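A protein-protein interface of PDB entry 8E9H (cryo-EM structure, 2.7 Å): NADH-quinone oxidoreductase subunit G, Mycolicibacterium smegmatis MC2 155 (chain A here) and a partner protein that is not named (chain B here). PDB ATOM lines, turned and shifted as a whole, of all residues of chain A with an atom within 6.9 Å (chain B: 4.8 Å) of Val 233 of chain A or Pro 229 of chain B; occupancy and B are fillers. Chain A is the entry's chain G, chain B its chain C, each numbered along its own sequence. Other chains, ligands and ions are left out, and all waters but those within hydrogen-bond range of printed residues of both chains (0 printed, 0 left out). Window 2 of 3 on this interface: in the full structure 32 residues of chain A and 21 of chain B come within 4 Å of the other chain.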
ATOM      1  N   PRO A 229      23.553  34.974  17.474  1.00  0.00           N
ATOM      2  CA  PRO A 229      22.518  35.662  16.693  1.00  0.00           C
ATOM      3  C   PRO A 229      22.490  35.261  15.233  1.00  0.00           C
ATOM      4  O   PRO A 229      21.407  35.134  14.652  1.00  0.00           O
ATOM      5  CB  PRO A 229      22.885  37.138  16.869  1.00  0.00           C
ATOM      6  CG  PRO A 229      23.569  37.190  18.169  1.00  0.00           C
ATOM      7  CD  PRO A 229      24.332  35.911  18.295  1.00  0.00           C
ATOM      8  N   PHE A 230      23.649  35.037  14.620  1.00  0.00           N
ATOM      9  CA  PHE A 230      23.690  34.838  13.178  1.00  0.00           C
ATOM     10  C   PHE A 230      22.961  33.580  12.728  1.00  0.00           C
ATOM     11  O   PHE A 230      22.388  33.581  11.636  1.00  0.00           O
ATOM     12  CB  PHE A 230      25.137  34.805  12.696  1.00  0.00           C
ATOM     13  CG  PHE A 230      25.793  33.470  12.832  1.00  0.00           C
ATOM     14  CD1 PHE A 230      26.343  33.079  14.035  1.00  0.00           C
ATOM     15  CD2 PHE A 230      25.862  32.606  11.760  1.00  0.00           C
ATOM     16  CE1 PHE A 230      26.949  31.856  14.165  1.00  0.00           C
ATOM     17  CE2 PHE A 230      26.468  31.381  11.888  1.00  0.00           C
ATOM     18  CZ  PHE A 230      27.010  31.007  13.091  1.00  0.00           C
ATOM     19  N   ASP A 231      22.966  32.514  13.523  1.00  0.00           N
ATOM     20  CA  ASP A 231      22.330  31.276  13.092  1.00  0.00           C
ATOM     21  C   ASP A 231      20.890  31.142  13.562  1.00  0.00           C
ATOM     22  O   ASP A 231      20.274  30.099  13.326  1.00  0.00           O
ATOM     23  CB  ASP A 231      23.132  30.063  13.571  1.00  0.00           C
ATOM     24  CG  ASP A 231      23.388  30.085  15.049  1.00  0.00           C
ATOM     25  OD1 ASP A 231      22.575  30.688  15.771  1.00  0.00           O
ATOM     26  OD2 ASP A 231      24.391  29.493  15.492  1.00  0.00           O
ATOM     27  N   LEU A 232      20.339  32.159  14.216  1.00  0.00           N
ATOM     28  CA  LEU A 232      18.943  32.114  14.618  1.00  0.00           C
ATOM     29  C   LEU A 232      18.042  32.550  13.476  1.00  0.00           C
ATOM     30  O   LEU A 232      18.291  33.569  12.830  1.00  0.00           O
ATOM     31  CB  LEU A 232      18.702  33.018  15.821  1.00  0.00           C
ATOM     32  CG  LEU A 232      19.458  32.668  17.090  1.00  0.00           C
ATOM     33  CD1 LEU A 232      19.323  33.792  18.091  1.00  0.00           C
ATOM     34  CD2 LEU A 232      18.930  31.377  17.662  1.00  0.00           C
ATOM     35  N   VAL A 233      16.993  31.784  13.231  1.00  0.00           N
ATOM     36  CA  VAL A 233      15.880  32.270  12.431  1.00  0.00           C
ATOM     37  C   VAL A 233      14.887  32.928  13.372  1.00  0.00           C
ATOM     38  O   VAL A 233      14.362  32.290  14.292  1.00  0.00           O
ATOM     39  CB  VAL A 233      15.232  31.127  11.636  1.00  0.00           C
ATOM     40  CG1 VAL A 233      14.038  31.640  10.857  1.00  0.00           C
ATOM     41  CG2 VAL A 233      16.239  30.498  10.703  1.00  0.00           C
ATOM     42  N   SER A 234      14.640  34.215  13.156  1.00  0.00           N
ATOM     43  CA  SER A 234      13.858  35.014  14.092  1.00  0.00           C
ATOM     44  C   SER A 234      12.613  35.507  13.379  1.00  0.00           C
ATOM     45  O   SER A 234      12.711  36.061  12.281  1.00  0.00           O
ATOM     46  CB  SER A 234      14.681  36.188  14.617  1.00  0.00           C
ATOM     47  OG  SER A 234      14.021  36.833  15.686  1.00  0.00           O
ATOM     48  N   SER A 235      11.453  35.307  13.994  1.00  0.00           N
ATOM     49  CA  SER A 235      10.203  35.703  13.373  1.00  0.00           C
ATOM     50  C   SER A 235       9.312  36.427  14.371  1.00  0.00           C
ATOM     51  O   SER A 235       9.279  36.061  15.549  1.00  0.00           O
ATOM     52  CB  SER A 235       9.461  34.479  12.825  1.00  0.00           C
ATOM     53  OG  SER A 235      10.272  33.757  11.917  1.00  0.00           O
ATOM     54  N   THR A 250      10.173  35.061  18.105  1.00  0.00           N
ATOM     55  CA  THR A 250      10.549  33.669  18.288  1.00  0.00           C
ATOM     56  C   THR A 250      11.850  33.405  17.548  1.00  0.00           C
ATOM     57  O   THR A 250      11.927  33.620  16.334  1.00  0.00           O
ATOM     58  CB  THR A 250       9.444  32.755  17.768  1.00  0.00           C
ATOM     59  OG1 THR A 250       8.235  32.999  18.495  1.00  0.00           O
ATOM     60  CG2 THR A 250       9.837  31.305  17.921  1.00  0.00           C
ATOM     61  N   ASP A 251      12.867  32.948  18.270  1.00  0.00           N
ATOM     62  CA  ASP A 251      14.159  32.612  17.694  1.00  0.00           C
ATOM     63  C   ASP A 251      14.338  31.106  17.745  1.00  0.00           C
ATOM     64  O   ASP A 251      14.295  30.514  18.828  1.00  0.00           O
ATOM     65  CB  ASP A 251      15.293  33.293  18.460  1.00  0.00           C
ATOM     66  CG  ASP A 251      15.214  34.797  18.398  1.00  0.00           C
ATOM     67  OD1 ASP A 251      14.450  35.319  17.565  1.00  0.00           O
ATOM     68  OD2 ASP A 251      15.918  35.460  19.187  1.00  0.00           O
ATOM     69  N   HIS A 252      14.538  30.486  16.588  1.00  0.00           N
ATOM     70  CA  HIS A 252      14.732  29.048  16.530  1.00  0.00           C
ATOM     71  C   HIS A 252      15.959  28.721  15.698  1.00  0.00           C
ATOM     72  O   HIS A 252      16.274  29.410  14.727  1.00  0.00           O
ATOM     73  CB  HIS A 252      13.510  28.327  15.951  1.00  0.00           C
ATOM     74  CG  HIS A 252      13.153  28.750  14.565  1.00  0.00           C
ATOM     75  ND1 HIS A 252      12.371  29.853  14.302  1.00  0.00           N
ATOM     76  CD2 HIS A 252      13.461  28.213  13.362  1.00  0.00           C
ATOM     77  CE1 HIS A 252      12.215  29.978  12.998  1.00  0.00           C
ATOM     78  NE2 HIS A 252      12.866  28.995  12.404  1.00  0.00           N
ATOM     79  N   ARG A 253      16.652  27.665  16.104  1.00  0.00           N
ATOM     80  CA  ARG A 253      17.826  27.166  15.408  1.00  0.00           C
ATOM     81  C   ARG A 253      17.584  25.722  15.010  1.00  0.00           C
ATOM     82  O   ARG A 253      17.054  24.933  15.796  1.00  0.00           O
ATOM     83  CB  ARG A 253      19.073  27.259  16.280  1.00  0.00           C
ATOM     84  CG  ARG A 253      20.359  26.984  15.538  1.00  0.00           C
ATOM     85  CD  ARG A 253      21.475  26.625  16.487  1.00  0.00           C
ATOM     86  NE  ARG A 253      22.723  26.379  15.776  1.00  0.00           N
ATOM     87  CZ  ARG A 253      23.929  26.619  16.268  1.00  0.00           C
ATOM     88  NH1 ARG A 253      24.098  27.089  17.491  1.00  0.00           N
ATOM     89  NH2 ARG A 253      24.996  26.379  15.513  1.00  0.00           N
ATOM     90  N   ARG A 254      17.974  25.384  13.784  1.00  0.00           N
ATOM     91  CA  ARG A 254      17.789  24.040  13.241  1.00  0.00           C
ATOM     92  C   ARG A 254      16.398  23.496  13.552  1.00  0.00           C
ATOM     93  O   ARG A 254      16.234  22.320  13.879  1.00  0.00           O
ATOM     94  CB  ARG A 254      18.872  23.082  13.746  1.00  0.00           C
ATOM     95  CG  ARG A 254      18.798  22.721  15.220  1.00  0.00           C
ATOM     96  CD  ARG A 254      19.524  21.415  15.485  1.00  0.00           C
ATOM     97  NE  ARG A 254      19.274  20.903  16.825  1.00  0.00           N
ATOM     98  CZ  ARG A 254      19.869  21.348  17.922  1.00  0.00           C
ATOM     99  NH1 ARG A 254      20.767  22.318  17.877  1.00  0.00           N
ATOM    100  NH2 ARG A 254      19.556  20.806  19.094  1.00  0.00           N
ATOM    101  N   GLY A 255      15.385  24.349  13.449  1.00  0.00           N
ATOM    102  CA  GLY A 255      14.016  23.900  13.590  1.00  0.00           C
ATOM    103  C   GLY A 255      13.532  23.727  15.009  1.00  0.00           C
ATOM    104  O   GLY A 255      12.439  23.190  15.211  1.00  0.00           O
ATOM    105  N   SER A 630       6.638  30.552  11.833  1.00  0.00           N
ATOM    106  CA  SER A 630       8.079  30.686  11.988  1.00  0.00           C
ATOM    107  C   SER A 630       8.802  29.458  11.456  1.00  0.00           C
ATOM    108  O   SER A 630       9.834  29.578  10.789  1.00  0.00           O
ATOM    109  CB  SER A 630       8.429  30.916  13.458  1.00  0.00           C
ATOM    110  OG  SER A 630       8.040  29.806  14.244  1.00  0.00           O
ATOM    111  N   LEU A 631       8.268  28.273  11.736  1.00  0.00           N
ATOM    112  CA  LEU A 631       8.846  27.016  11.269  1.00  0.00           C
ATOM    113  C   LEU A 631       8.032  26.525  10.082  1.00  0.00           C
ATOM    114  O   LEU A 631       6.866  26.152  10.225  1.00  0.00           O
ATOM    115  CB  LEU A 631       8.858  25.985  12.389  1.00  0.00           C
ATOM    116  CG  LEU A 631      10.036  26.057  13.353  1.00  0.00           C
ATOM    117  CD1 LEU A 631       9.957  27.315  14.184  1.00  0.00           C
ATOM    118  CD2 LEU A 631      10.059  24.834  14.244  1.00  0.00           C
ATOM    119  N   PRO B 220      18.460  24.934   2.721  1.00  0.00           N
ATOM    120  CA  PRO B 220      19.230  24.700   3.944  1.00  0.00           C
ATOM    121  C   PRO B 220      20.462  23.857   3.664  1.00  0.00           C
ATOM    122  O   PRO B 220      20.428  22.914   2.873  1.00  0.00           O
ATOM    123  CB  PRO B 220      18.239  23.967   4.851  1.00  0.00           C
ATOM    124  CG  PRO B 220      16.903  24.308   4.315  1.00  0.00           C
ATOM    125  CD  PRO B 220      17.081  24.441   2.843  1.00  0.00           C
ATOM    126  N   GLN B 227      20.517  21.442  10.103  1.00  0.00           N
ATOM    127  CA  GLN B 227      20.679  22.146   8.844  1.00  0.00           C
ATOM    128  C   GLN B 227      20.633  23.642   9.101  1.00  0.00           C
ATOM    129  O   GLN B 227      19.927  24.115   9.993  1.00  0.00           O
ATOM    130  CB  GLN B 227      19.609  21.745   7.828  1.00  0.00           C
ATOM    131  CG  GLN B 227      18.194  21.991   8.281  1.00  0.00           C
ATOM    132  CD  GLN B 227      17.182  21.406   7.321  1.00  0.00           C
ATOM    133  OE1 GLN B 227      17.511  20.549   6.505  1.00  0.00           O
ATOM    134  NE2 GLN B 227      15.943  21.870   7.412  1.00  0.00           N
ATOM    135  N   ILE B 228      21.397  24.378   8.307  1.00  0.00           N
ATOM    136  CA  ILE B 228      21.524  25.826   8.440  1.00  0.00           C
ATOM    137  C   ILE B 228      20.698  26.475   7.336  1.00  0.00           C
ATOM    138  O   ILE B 228      21.068  26.359   6.161  1.00  0.00           O
ATOM    139  CB  ILE B 228      22.990  26.272   8.356  1.00  0.00           C
ATOM    140  CG1 ILE B 228      23.810  25.593   9.449  1.00  0.00           C
ATOM    141  CG2 ILE B 228      23.089  27.780   8.490  1.00  0.00           C
ATOM    142  CD1 ILE B 228      25.270  25.941   9.414  1.00  0.00           C
ATOM    143  N   PRO B 229      19.614  27.172   7.654  1.00  0.00           N
ATOM    144  CA  PRO B 229      18.827  27.820   6.609  1.00  0.00           C
ATOM    145  C   PRO B 229      19.678  28.786   5.808  1.00  0.00           C
ATOM    146  O   PRO B 229      20.780  29.156   6.235  1.00  0.00           O
ATOM    147  CB  PRO B 229      17.739  28.560   7.399  1.00  0.00           C
ATOM    148  CG  PRO B 229      17.625  27.804   8.655  1.00  0.00           C
ATOM    149  CD  PRO B 229      19.011  27.366   8.980  1.00  0.00           C
ATOM    150  N   PRO B 230      19.205  29.219   4.646  1.00  0.00           N
ATOM    151  CA  PRO B 230      19.969  30.172   3.847  1.00  0.00           C
ATOM    152  C   PRO B 230      20.160  31.472   4.605  1.00  0.00           C
ATOM    153  O   PRO B 230      19.358  31.809   5.486  1.00  0.00           O
ATOM    154  CB  PRO B 230      19.093  30.374   2.604  1.00  0.00           C
ATOM    155  CG  PRO B 230      18.231  29.179   2.549  1.00  0.00           C
ATOM    156  CD  PRO B 230      17.968  28.810   3.968  1.00  0.00           C
ATOM    157  N   PRO B 231      21.206  32.236   4.286  1.00  0.00           N
ATOM    158  CA  PRO B 231      21.500  33.443   5.069  1.00  0.00           C
ATOM    159  C   PRO B 231      20.379  34.461   5.073  1.00  0.00           C
ATOM    160  O   PRO B 231      20.287  35.243   6.027  1.00  0.00           O
ATOM    161  CB  PRO B 231      22.749  34.001   4.384  1.00  0.00           C
ATOM    162  CG  PRO B 231      22.643  33.512   2.989  1.00  0.00           C
ATOM    163  CD  PRO B 231      22.071  32.135   3.101  1.00  0.00           C
ATOM    164  N   GLN B 233      17.166  33.904   5.415  1.00  0.00           N
ATOM    165  CA  GLN B 233      16.200  33.575   6.454  1.00  0.00           C
ATOM    166  C   GLN B 233      16.737  33.870   7.844  1.00  0.00           C
ATOM    167  O   GLN B 233      15.968  34.232   8.737  1.00  0.00           O
ATOM    168  CB  GLN B 233      15.816  32.102   6.362  1.00  0.00           C
ATOM    169  CG  GLN B 233      15.238  31.702   5.030  1.00  0.00           C
ATOM    170  CD  GLN B 233      14.740  30.279   5.032  1.00  0.00           C
ATOM    171  OE1 GLN B 233      14.687  29.633   6.076  1.00  0.00           O
ATOM    172  NE2 GLN B 233      14.377  29.779   3.860  1.00  0.00           N
ATOM    173  N   ARG B 234      18.040  33.722   8.045  1.00  0.00           N
ATOM    174  CA  ARG B 234      18.617  33.865   9.366  1.00  0.00           C
ATOM    175  C   ARG B 234      18.769  35.336   9.731  1.00  0.00           C
ATOM    176  O   ARG B 234      18.520  36.240   8.931  1.00  0.00           O
ATOM    177  CB  ARG B 234      19.963  33.152   9.433  1.00  0.00           C
ATOM    178  CG  ARG B 234      19.887  31.711   8.983  1.00  0.00           C
ATOM    179  CD  ARG B 234      21.113  30.930   9.381  1.00  0.00           C
ATOM    180  NE  ARG B 234      22.338  31.667   9.108  1.00  0.00           N
ATOM    181  CZ  ARG B 234      23.020  31.596   7.974  1.00  0.00           C
ATOM    182  NH1 ARG B 234      22.610  30.844   6.966  1.00  0.00           N
ATOM    183  NH2 ARG B 234      24.139  32.301   7.845  1.00  0.00           N
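Among the printed residues, pairs that only touch across the chains: Asp 231 of chain A with Arg 234 of chain B (3.9 Å), Leu 232 of chain A with Arg 234 of chain B (3.5 Å), Val 233 of chain A with Pro 229 of chain B (3.7 Å), Val 233 of chain A with Gln 233 of chain B (3.9 Å) and Arg 254 of chain A with Gln 227 of chain B (3.9 Å).
O of Pro 229 of chain B is in hydrogen-bond range of NH1 of Arg 234 of chain B (2.6 Å).
The side-chain carboxylate (OD2) of Asp 231 of chain A is in salt-bridge range of the guanidinium group (NH1) of Arg 253 of chain A, at 3.1 Å.
The backbone NH of Val 233 of chain A sits at hydrogen-bond distance from the backbone carbonyl oxygen of His 252 of chain A (2.9 Å).
Of the 15 printed residues of chain A, 5 touch a printed residue of chain B.
Printed residues of chain A that touch a printed residue of chain B: Phe 230, Asp 231, Leu 232, Val 233 and Arg 254.
Hydrophobic or aromatic side chains of chain A that line the printed part of chain B: Val 233.
Along chain A the printed residues that touch a printed residue of chain B span positions 230 to 254.
Among the printed residues, no Asp or Glu carboxylate lies within 4 Å of a Lys or Arg side-chain nitrogen of the other chain.
The backbone carbonyl oxygen of Phe 230 of chain A lies within hydrogen-bond range of the guanidinium group of Arg 234 of chain B (3.2 Å).
Val 233 of chain A touches two residues of chain B.
Pro 229 of chain B touches one residue of chain A.
Of the printed residues of chain A, Gln 233 of chain B touches Val 233.
Of the printed residues of chain A, Gln 227 of chain B touches Arg 254 (3.9 Å).
Of the printed residues of chain B, Phe 230 of chain A touches Arg 234.
The nearest residue of chain B that does not touch Val 233 of chain A is Arg 234 of chain B (4.2 Å).
The nearest printed residue of chain B that does not touch Arg 254 of chain A is Pro 229 of chain B (5.3 Å).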
